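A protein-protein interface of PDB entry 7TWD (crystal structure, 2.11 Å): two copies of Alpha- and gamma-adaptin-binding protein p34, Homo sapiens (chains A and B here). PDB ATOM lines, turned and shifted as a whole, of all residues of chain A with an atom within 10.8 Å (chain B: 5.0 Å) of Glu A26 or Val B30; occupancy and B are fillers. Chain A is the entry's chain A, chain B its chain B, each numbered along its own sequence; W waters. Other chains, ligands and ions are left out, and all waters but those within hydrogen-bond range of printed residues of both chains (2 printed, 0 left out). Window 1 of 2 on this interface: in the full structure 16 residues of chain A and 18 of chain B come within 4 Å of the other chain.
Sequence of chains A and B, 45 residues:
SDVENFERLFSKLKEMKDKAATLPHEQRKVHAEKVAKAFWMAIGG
The side-chain carboxylate (OE2) of Glu A26 sits close to the side-chain carboxylate (OE1) of Glu B26, at 2.7 Å. OE2 of Glu A26 is in salt-bridge range of NZ of Lys B29 (3.5 Å).
The side-chain hydroxyl of Thr A22 lies within hydrogen-bond range of the backbone carbonyl oxygen of Asp A18. The backbone carbonyl oxygen of Leu A23 lies close to the side-chain amide oxygen of Gln A27 (3.4 Å).
Among the printed residues, merely in contact across the chains: Glu A33 with Glu B26 (3.1 Å), Lys A29 with Glu B26 (3.2 Å), Glu A26 with Glu B33 (3.2 Å), Lys A19 with Glu B33 (3.3 Å), Lys A34 with Gln B27 (3.5 Å), Leu A23 with Glu B33 (3.6 Å), Val A30 with Val B30 (3.6 Å), Glu A26 with Val B30 (3.7 Å), Leu A23 with Lys B34 (3.8 Å), Val A30 with Glu B26 (3.8 Å), Leu A23 with Val B30 (3.9 Å) and Thr A22 with Glu B33 (3.95 Å).
Glu A26 touches just these residues of chain B: Glu B26, Lys B29, Val B30 and Glu B33. Printed residues of chain A within 4 Å of Val B30: Leu A23, Glu A26 and Val A30. Of chain A, only Glu A26 (3.2 Å) comes within 4 Å of Lys B29. Printed residues of chain B within 4 Å of Lys A29: Glu B26. Of the printed residues of chain B, Lys A34 touches Gln B27. Of the printed residues of chain B, Glu A33 touches Glu B26 (3.1 Å). Ala A32 touches none of the printed residues of chain B. His A25 touches none of the printed residues of chain B. The nearest residue of chain A that does not touch Val B30 is Gln A27 (4.2 Å). The nearest printed residue of chain A that does not touch Gln B27 is Val A30 (4.3 Å).
Hydrophobic or aromatic side chains of chain A that line the printed part of chain B: Leu A23 and Val A30. Among the printed residues, Asp or Glu carboxylates within 4 Å of a Lys or Arg side-chain nitrogen of the other chain: Glu A26 with Lys B29 (3.5 Å).
Glu A26 touches its own counterpart, Glu B26. Glu A26 touches Lys B29, and with the chains exchanged Lys A29 touches Glu B26. Glu A26 touches Glu B33, and with the chains exchanged Glu A33 touches Glu B26. Lys A34 touches Gln B27, but with the chains exchanged Gln A27 does not touch Lys B34 (4.01 Å). Positions printed for both chains: 26, 27, 28, 29, 30, 31, 32, 33 and 34.
Water W1 lies within hydrogen-bond range of the side-chain amide nitrogen of Gln B27 (2.7 Å) and the side-chain amino group of Lys A34 (2.8 Å). Water W2 bridges the side-chain amide nitrogen of Gln A27 (2.7 Å) and the side-chain amino group of Lys B34 (3.2 Å).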
ATOM      1  N   MET A  16       1.794  35.982  24.196  1.00  0.00           N
ATOM      2  CA  MET A  16       1.144  35.125  25.180  1.00  0.00           C
ATOM      3  C   MET A  16      -0.348  34.998  24.898  1.00  0.00           C
ATOM      4  O   MET A  16      -0.925  33.913  25.044  1.00  0.00           O
ATOM      5  CB  MET A  16       1.391  35.681  26.583  1.00  0.00           C
ATOM      6  CG  MET A  16       0.708  34.928  27.708  1.00  0.00           C
ATOM      7  SD  MET A  16       0.902  35.804  29.272  1.00  0.00           S
ATOM      8  CE  MET A  16       2.687  35.897  29.370  1.00  0.00           C
ATOM      9  N   ASP A  18      -1.681  35.203  21.902  1.00  0.00           N
ATOM     10  CA  ASP A  18      -1.828  34.396  20.695  1.00  0.00           C
ATOM     11  C   ASP A  18      -1.613  32.916  20.987  1.00  0.00           C
ATOM     12  O   ASP A  18      -2.345  32.064  20.468  1.00  0.00           O
ATOM     13  CB  ASP A  18      -0.854  34.884  19.624  1.00  0.00           C
ATOM     14  CG  ASP A  18      -1.234  36.243  19.067  1.00  0.00           C
ATOM     15  OD1 ASP A  18      -2.413  36.635  19.202  1.00  0.00           O
ATOM     16  OD2 ASP A  18      -0.353  36.924  18.500  1.00  0.00           O
ATOM     17  N   LYS A  19      -0.611  32.589  21.807  1.00  0.00           N
ATOM     18  CA  LYS A  19      -0.405  31.200  22.207  1.00  0.00           C
ATOM     19  C   LYS A  19      -1.630  30.657  22.930  1.00  0.00           C
ATOM     20  O   LYS A  19      -2.107  29.556  22.631  1.00  0.00           O
ATOM     21  CB  LYS A  19       0.828  31.084  23.103  1.00  0.00           C
ATOM     22  CG  LYS A  19       2.162  31.273  22.408  1.00  0.00           C
ATOM     23  CD  LYS A  19       3.271  31.332  23.448  1.00  0.00           C
ATOM     24  CE  LYS A  19       4.642  31.107  22.844  1.00  0.00           C
ATOM     25  NZ  LYS A  19       5.694  31.113  23.901  1.00  0.00           N
ATOM     26  N   ALA A  20      -2.154  31.424  23.888  1.00  0.00           N
ATOM     27  CA  ALA A  20      -3.317  30.978  24.651  1.00  0.00           C
ATOM     28  C   ALA A  20      -4.530  30.780  23.750  1.00  0.00           C
ATOM     29  O   ALA A  20      -5.317  29.850  23.954  1.00  0.00           O
ATOM     30  CB  ALA A  20      -3.630  31.983  25.759  1.00  0.00           C
ATOM     31  N   ALA A  21      -4.696  31.644  22.745  1.00  0.00           N
ATOM     32  CA  ALA A  21      -5.852  31.531  21.863  1.00  0.00           C
ATOM     33  C   ALA A  21      -5.717  30.361  20.897  1.00  0.00           C
ATOM     34  O   ALA A  21      -6.728  29.793  20.470  1.00  0.00           O
ATOM     35  CB  ALA A  21      -6.054  32.836  21.093  1.00  0.00           C
ATOM     36  N   THR A  22      -4.488  29.985  20.546  1.00  0.00           N
ATOM     37  CA  THR A  22      -4.258  28.890  19.610  1.00  0.00           C
ATOM     38  C   THR A  22      -4.337  27.517  20.269  1.00  0.00           C
ATOM     39  O   THR A  22      -4.374  26.509  19.555  1.00  0.00           O
ATOM     40  CB  THR A  22      -2.892  29.065  18.935  1.00  0.00           C
ATOM     41  OG1 THR A  22      -2.663  30.454  18.675  1.00  0.00           O
ATOM     42  CG2 THR A  22      -2.833  28.306  17.615  1.00  0.00           C
ATOM     43  N   LEU A  23      -4.378  27.454  21.601  1.00  0.00           N
ATOM     44  CA  LEU A  23      -4.365  26.173  22.308  1.00  0.00           C
ATOM     45  C   LEU A  23      -5.449  25.201  21.851  1.00  0.00           C
ATOM     46  O   LEU A  23      -5.122  24.030  21.601  1.00  0.00           O
ATOM     47  CB  LEU A  23      -4.454  26.428  23.820  1.00  0.00           C
ATOM     48  CG  LEU A  23      -4.458  25.191  24.725  1.00  0.00           C
ATOM     49  CD1 LEU A  23      -3.251  24.306  24.442  1.00  0.00           C
ATOM     50  CD2 LEU A  23      -4.499  25.594  26.192  1.00  0.00           C
ATOM     51  N   PRO A  24      -6.727  25.588  21.724  1.00  0.00           N
ATOM     52  CA  PRO A  24      -7.725  24.599  21.275  1.00  0.00           C
ATOM     53  C   PRO A  24      -7.465  24.073  19.875  1.00  0.00           C
ATOM     54  O   PRO A  24      -7.652  22.876  19.624  1.00  0.00           O
ATOM     55  CB  PRO A  24      -9.049  25.373  21.357  1.00  0.00           C
ATOM     56  CG  PRO A  24      -8.783  26.497  22.297  1.00  0.00           C
ATOM     57  CD  PRO A  24      -7.361  26.879  22.048  1.00  0.00           C
ATOM     58  N   HIS A  25      -7.037  24.937  18.950  1.00  0.00           N
ATOM     59  CA  HIS A  25      -6.724  24.477  17.600  1.00  0.00           C
ATOM     60  C   HIS A  25      -5.535  23.525  17.601  1.00  0.00           C
ATOM     61  O   HIS A  25      -5.542  22.510  16.894  1.00  0.00           O
ATOM     62  CB  HIS A  25      -6.453  25.674  16.688  1.00  0.00           C
ATOM     63  CG  HIS A  25      -5.702  25.327  15.441  1.00  0.00           C
ATOM     64  ND1 HIS A  25      -6.301  24.732  14.352  1.00  0.00           N
ATOM     65  CD2 HIS A  25      -4.399  25.490  15.111  1.00  0.00           C
ATOM     66  CE1 HIS A  25      -5.401  24.544  13.405  1.00  0.00           C
ATOM     67  NE2 HIS A  25      -4.238  24.995  13.840  1.00  0.00           N
ATOM     68  N   GLU A  26      -4.505  23.831  18.392  1.00  0.00           N
ATOM     69  CA  GLU A  26      -3.321  22.977  18.429  1.00  0.00           C
ATOM     70  C   GLU A  26      -3.634  21.633  19.074  1.00  0.00           C
ATOM     71  O   GLU A  26      -3.078  20.602  18.676  1.00  0.00           O
ATOM     72  CB  GLU A  26      -2.196  23.684  19.181  1.00  0.00           C
ATOM     73  CG  GLU A  26      -0.806  23.386  18.663  1.00  0.00           C
ATOM     74  CD  GLU A  26      -0.512  24.135  17.378  1.00  0.00           C
ATOM     75  OE1 GLU A  26      -1.094  25.221  17.181  1.00  0.00           O
ATOM     76  OE2 GLU A  26       0.305  23.652  16.568  1.00  0.00           O
ATOM     77  N   GLN A  27      -4.520  21.625  20.074  1.00  0.00           N
ATOM     78  CA  GLN A  27      -4.943  20.363  20.674  1.00  0.00           C
ATOM     79  C   GLN A  27      -5.683  19.485  19.674  1.00  0.00           C
ATOM     80  O   GLN A  27      -5.577  18.254  19.731  1.00  0.00           O
ATOM     81  CB  GLN A  27      -5.822  20.628  21.897  1.00  0.00           C
ATOM     82  CG  GLN A  27      -5.059  21.140  23.106  1.00  0.00           C
ATOM     83  CD  GLN A  27      -5.975  21.504  24.257  1.00  0.00           C
ATOM     84  OE1 GLN A  27      -6.783  22.428  24.156  1.00  0.00           O
ATOM     85  NE2 GLN A  27      -5.854  20.776  25.359  1.00  0.00           N
ATOM     86  N   ARG A  28      -6.439  20.093  18.754  1.00  0.00           N
ATOM     87  CA  ARG A  28      -7.103  19.310  17.717  1.00  0.00           C
ATOM     88  C   ARG A  28      -6.101  18.770  16.706  1.00  0.00           C
ATOM     89  O   ARG A  28      -6.276  17.662  16.184  1.00  0.00           O
ATOM     90  CB  ARG A  28      -8.175  20.150  17.022  1.00  0.00           C
ATOM     91  CG  ARG A  28      -9.281  20.625  17.948  1.00  0.00           C
ATOM     92  CD  ARG A  28     -10.438  21.238  17.174  1.00  0.00           C
ATOM     93  NE  ARG A  28     -10.070  22.499  16.540  1.00  0.00           N
ATOM     94  CZ  ARG A  28     -10.303  23.692  17.076  1.00  0.00           C
ATOM     95  NH1 ARG A  28     -10.899  23.782  18.257  1.00  0.00           N
ATOM     96  NH2 ARG A  28      -9.937  24.797  16.438  1.00  0.00           N
ATOM     97  N   LYS A  29      -5.039  19.531  16.423  1.00  0.00           N
ATOM     98  CA  LYS A  29      -4.005  19.058  15.510  1.00  0.00           C
ATOM     99  C   LYS A  29      -3.240  17.886  16.114  1.00  0.00           C
ATOM    100  O   LYS A  29      -2.906  16.920  15.423  1.00  0.00           O
ATOM    101  CB  LYS A  29      -3.054  20.202  15.162  1.00  0.00           C
ATOM    102  CG  LYS A  29      -1.993  19.822  14.143  1.00  0.00           C
ATOM    103  CD  LYS A  29      -1.028  20.971  13.882  1.00  0.00           C
ATOM    104  CE  LYS A  29      -0.691  21.091  12.403  1.00  0.00           C
ATOM    105  NZ  LYS A  29      -0.744  22.506  11.937  1.00  0.00           N
ATOM    106  N   VAL A  30      -2.946  17.969  17.414  1.00  0.00           N
ATOM    107  CA  VAL A  30      -2.267  16.879  18.113  1.00  0.00           C
ATOM    108  C   VAL A  30      -3.114  15.611  18.073  1.00  0.00           C
ATOM    109  O   VAL A  30      -2.600  14.508  17.841  1.00  0.00           O
ATOM    110  CB  VAL A  30      -1.940  17.311  19.556  1.00  0.00           C
ATOM    111  CG1 VAL A  30      -1.701  16.100  20.444  1.00  0.00           C
ATOM    112  CG2 VAL A  30      -0.743  18.249  19.559  1.00  0.00           C
ATOM    113  N   HIS A  31      -4.423  15.745  18.295  1.00  0.00           N
ATOM    114  CA  HIS A  31      -5.300  14.581  18.244  1.00  0.00           C
ATOM    115  C   HIS A  31      -5.331  13.974  16.847  1.00  0.00           C
ATOM    116  O   HIS A  31      -5.253  12.751  16.693  1.00  0.00           O
ATOM    117  CB  HIS A  31      -6.711  14.960  18.695  1.00  0.00           C
ATOM    118  CG  HIS A  31      -7.698  13.842  18.575  1.00  0.00           C
ATOM    119  ND1 HIS A  31      -7.754  12.801  19.477  1.00  0.00           N
ATOM    120  CD2 HIS A  31      -8.656  13.591  17.651  1.00  0.00           C
ATOM    121  CE1 HIS A  31      -8.709  11.961  19.118  1.00  0.00           C
ATOM    122  NE2 HIS A  31      -9.271  12.418  18.013  1.00  0.00           N
ATOM    123  N   ALA A  32      -5.439  14.816  15.817  1.00  0.00           N
ATOM    124  CA  ALA A  32      -5.455  14.308  14.450  1.00  0.00           C
ATOM    125  C   ALA A  32      -4.133  13.640  14.097  1.00  0.00           C
ATOM    126  O   ALA A  32      -4.111  12.622  13.395  1.00  0.00           O
ATOM    127  CB  ALA A  32      -5.765  15.440  13.472  1.00  0.00           C
ATOM    128  N   GLU A  33      -3.017  14.197  14.574  1.00  0.00           N
ATOM    129  CA  GLU A  33      -1.720  13.587  14.302  1.00  0.00           C
ATOM    130  C   GLU A  33      -1.555  12.271  15.048  1.00  0.00           C
ATOM    131  O   GLU A  33      -0.910  11.348  14.537  1.00  0.00           O
ATOM    132  CB  GLU A  33      -0.598  14.553  14.673  1.00  0.00           C
ATOM    133  CG  GLU A  33      -0.375  15.658  13.658  1.00  0.00           C
ATOM    134  CD  GLU A  33       0.468  16.783  14.215  1.00  0.00           C
ATOM    135  OE1 GLU A  33       0.572  17.840  13.557  1.00  0.00           O
ATOM    136  OE2 GLU A  33       1.021  16.607  15.320  1.00  0.00           O
ATOM    137  N   LYS A  34      -2.127  12.165  16.250  1.00  0.00           N
ATOM    138  CA  LYS A  34      -2.100  10.897  16.970  1.00  0.00           C
ATOM    139  C   LYS A  34      -2.916   9.835  16.243  1.00  0.00           C
ATOM    140  O   LYS A  34      -2.514   8.668  16.184  1.00  0.00           O
ATOM    141  CB  LYS A  34      -2.618  11.093  18.393  1.00  0.00           C
ATOM    142  CG  LYS A  34      -1.637  11.755  19.345  1.00  0.00           C
ATOM    143  CD  LYS A  34      -2.262  11.928  20.718  1.00  0.00           C
ATOM    144  CE  LYS A  34      -1.267  12.477  21.724  1.00  0.00           C
ATOM    145  NZ  LYS A  34      -1.914  12.728  23.042  1.00  0.00           N
ATOM    146  N   GLU B  26       4.647  19.121  17.914  1.00  0.00           N
ATOM    147  CA  GLU B  26       3.307  19.624  18.192  1.00  0.00           C
ATOM    148  C   GLU B  26       2.975  19.536  19.674  1.00  0.00           C
ATOM    149  O   GLU B  26       2.302  20.419  20.219  1.00  0.00           O
ATOM    150  CB  GLU B  26       2.290  18.846  17.364  1.00  0.00           C
ATOM    151  CG  GLU B  26       2.101  19.436  15.994  1.00  0.00           C
ATOM    152  CD  GLU B  26       1.432  20.785  16.058  1.00  0.00           C
ATOM    153  OE1 GLU B  26       0.552  20.961  16.928  1.00  0.00           O
ATOM    154  OE2 GLU B  26       1.791  21.667  15.250  1.00  0.00           O
ATOM    155  N   GLN B  27       3.437  18.478  20.341  1.00  0.00           N
ATOM    156  CA  GLN B  27       3.166  18.325  21.764  1.00  0.00           C
ATOM    157  C   GLN B  27       3.965  19.319  22.598  1.00  0.00           C
ATOM    158  O   GLN B  27       3.482  19.781  23.638  1.00  0.00           O
ATOM    159  CB  GLN B  27       3.463  16.890  22.196  1.00  0.00           C
ATOM    160  CG  GLN B  27       2.317  15.923  21.930  1.00  0.00           C
ATOM    161  CD  GLN B  27       2.740  14.470  22.013  1.00  0.00           C
ATOM    162  OE1 GLN B  27       3.809  14.093  21.534  1.00  0.00           O
ATOM    163  NE2 GLN B  27       1.899  13.644  22.627  1.00  0.00           N
ATOM    164  N   ARG B  28       5.181  19.661  22.163  1.00  0.00           N
ATOM    165  CA  ARG B  28       5.940  20.702  22.847  1.00  0.00           C
ATOM    166  C   ARG B  28       5.279  22.062  22.672  1.00  0.00           C
ATOM    167  O   ARG B  28       5.264  22.879  23.600  1.00  0.00           O
ATOM    168  CB  ARG B  28       7.378  20.734  22.328  1.00  0.00           C
ATOM    169  CG  ARG B  28       8.222  19.533  22.728  1.00  0.00           C
ATOM    170  CD  ARG B  28       9.681  19.727  22.333  1.00  0.00           C
ATOM    171  NE  ARG B  28       9.871  19.701  20.885  1.00  0.00           N
ATOM    172  CZ  ARG B  28      10.230  18.621  20.196  1.00  0.00           C
ATOM    173  NH1 ARG B  28      10.438  17.472  20.822  1.00  0.00           N
ATOM    174  NH2 ARG B  28      10.379  18.691  18.880  1.00  0.00           N
ATOM    175  N   LYS B  29       4.727  22.320  21.485  1.00  0.00           N
ATOM    176  CA  LYS B  29       4.028  23.577  21.245  1.00  0.00           C
ATOM    177  C   LYS B  29       2.762  23.674  22.090  1.00  0.00           C
ATOM    178  O   LYS B  29       2.417  24.756  22.579  1.00  0.00           O
ATOM    179  CB  LYS B  29       3.702  23.702  19.758  1.00  0.00           C
ATOM    180  CG  LYS B  29       3.223  25.067  19.312  1.00  0.00           C
ATOM    181  CD  LYS B  29       2.872  25.037  17.834  1.00  0.00           C
ATOM    182  CE  LYS B  29       3.112  26.380  17.171  1.00  0.00           C
ATOM    183  NZ  LYS B  29       2.151  26.615  16.058  1.00  0.00           N
ATOM    184  N   VAL B  30       2.066  22.551  22.283  1.00  0.00           N
ATOM    185  CA  VAL B  30       0.859  22.553  23.107  1.00  0.00           C
ATOM    186  C   VAL B  30       1.206  22.844  24.561  1.00  0.00           C
ATOM    187  O   VAL B  30       0.487  23.575  25.253  1.00  0.00           O
ATOM    188  CB  VAL B  30       0.108  21.215  22.957  1.00  0.00           C
ATOM    189  CG1 VAL B  30      -0.792  20.963  24.158  1.00  0.00           C
ATOM    190  CG2 VAL B  30      -0.710  21.209  21.678  1.00  0.00           C
ATOM    191  N   HIS B  31       2.314  22.281  25.047  1.00  0.00           N
ATOM    192  CA  HIS B  31       2.728  22.540  26.422  1.00  0.00           C
ATOM    193  C   HIS B  31       3.056  24.013  26.629  1.00  0.00           C
ATOM    194  O   HIS B  31       2.663  24.615  27.635  1.00  0.00           O
ATOM    195  CB  HIS B  31       3.931  21.668  26.784  1.00  0.00           C
ATOM    196  CG  HIS B  31       4.563  22.034  28.088  1.00  0.00           C
ATOM    197  ND1 HIS B  31       3.963  21.785  29.303  1.00  0.00           N
ATOM    198  CD2 HIS B  31       5.736  22.652  28.367  1.00  0.00           C
ATOM    199  CE1 HIS B  31       4.743  22.223  30.275  1.00  0.00           C
ATOM    200  NE2 HIS B  31       5.825  22.753  29.734  1.00  0.00           N
ATOM    201  N   ALA B  32       3.783  24.611  25.681  1.00  0.00           N
ATOM    202  CA  ALA B  32       4.117  26.027  25.787  1.00  0.00           C
ATOM    203  C   ALA B  32       2.864  26.895  25.768  1.00  0.00           C
ATOM    204  O   ALA B  32       2.792  27.912  26.466  1.00  0.00           O
ATOM    205  CB  ALA B  32       5.066  26.427  24.657  1.00  0.00           C
ATOM    206  N   GLU B  33       1.861  26.502  24.977  1.00  0.00           N
ATOM    207  CA  GLU B  33       0.621  27.266  24.919  1.00  0.00           C
ATOM    208  C   GLU B  33      -0.214  27.083  26.180  1.00  0.00           C
ATOM    209  O   GLU B  33      -0.916  28.010  26.598  1.00  0.00           O
ATOM    210  CB  GLU B  33      -0.181  26.866  23.681  1.00  0.00           C
ATOM    211  CG  GLU B  33       0.385  27.412  22.379  1.00  0.00           C
ATOM    212  CD  GLU B  33      -0.115  26.658  21.162  1.00  0.00           C
ATOM    213  OE1 GLU B  33      -0.919  25.719  21.333  1.00  0.00           O
ATOM    214  OE2 GLU B  33       0.295  27.006  20.034  1.00  0.00           O
ATOM    215  N   LYS B  34      -0.157  25.897  26.794  1.00  0.00           N
ATOM    216  CA  LYS B  34      -0.818  25.703  28.082  1.00  0.00           C
ATOM    217  C   LYS B  34      -0.188  26.580  29.155  1.00  0.00           C
ATOM    218  O   LYS B  34      -0.895  27.175  29.977  1.00  0.00           O
ATOM    219  CB  LYS B  34      -0.751  24.232  28.493  1.00  0.00           C
ATOM    220  CG  LYS B  34      -1.671  23.313  27.708  1.00  0.00           C
ATOM    221  CD  LYS B  34      -1.473  21.871  28.141  1.00  0.00           C
ATOM    222  CE  LYS B  34      -2.409  20.931  27.400  1.00  0.00           C
ATOM    223  NZ  LYS B  34      -2.142  19.508  27.744  1.00  0.00           N
HETATM  224  O   HOH W   1      -0.130  14.654  24.027  1.00  0.00           O
HETATM  225  O   HOH W   2      -4.285  18.598  25.569  1.00  0.00           O
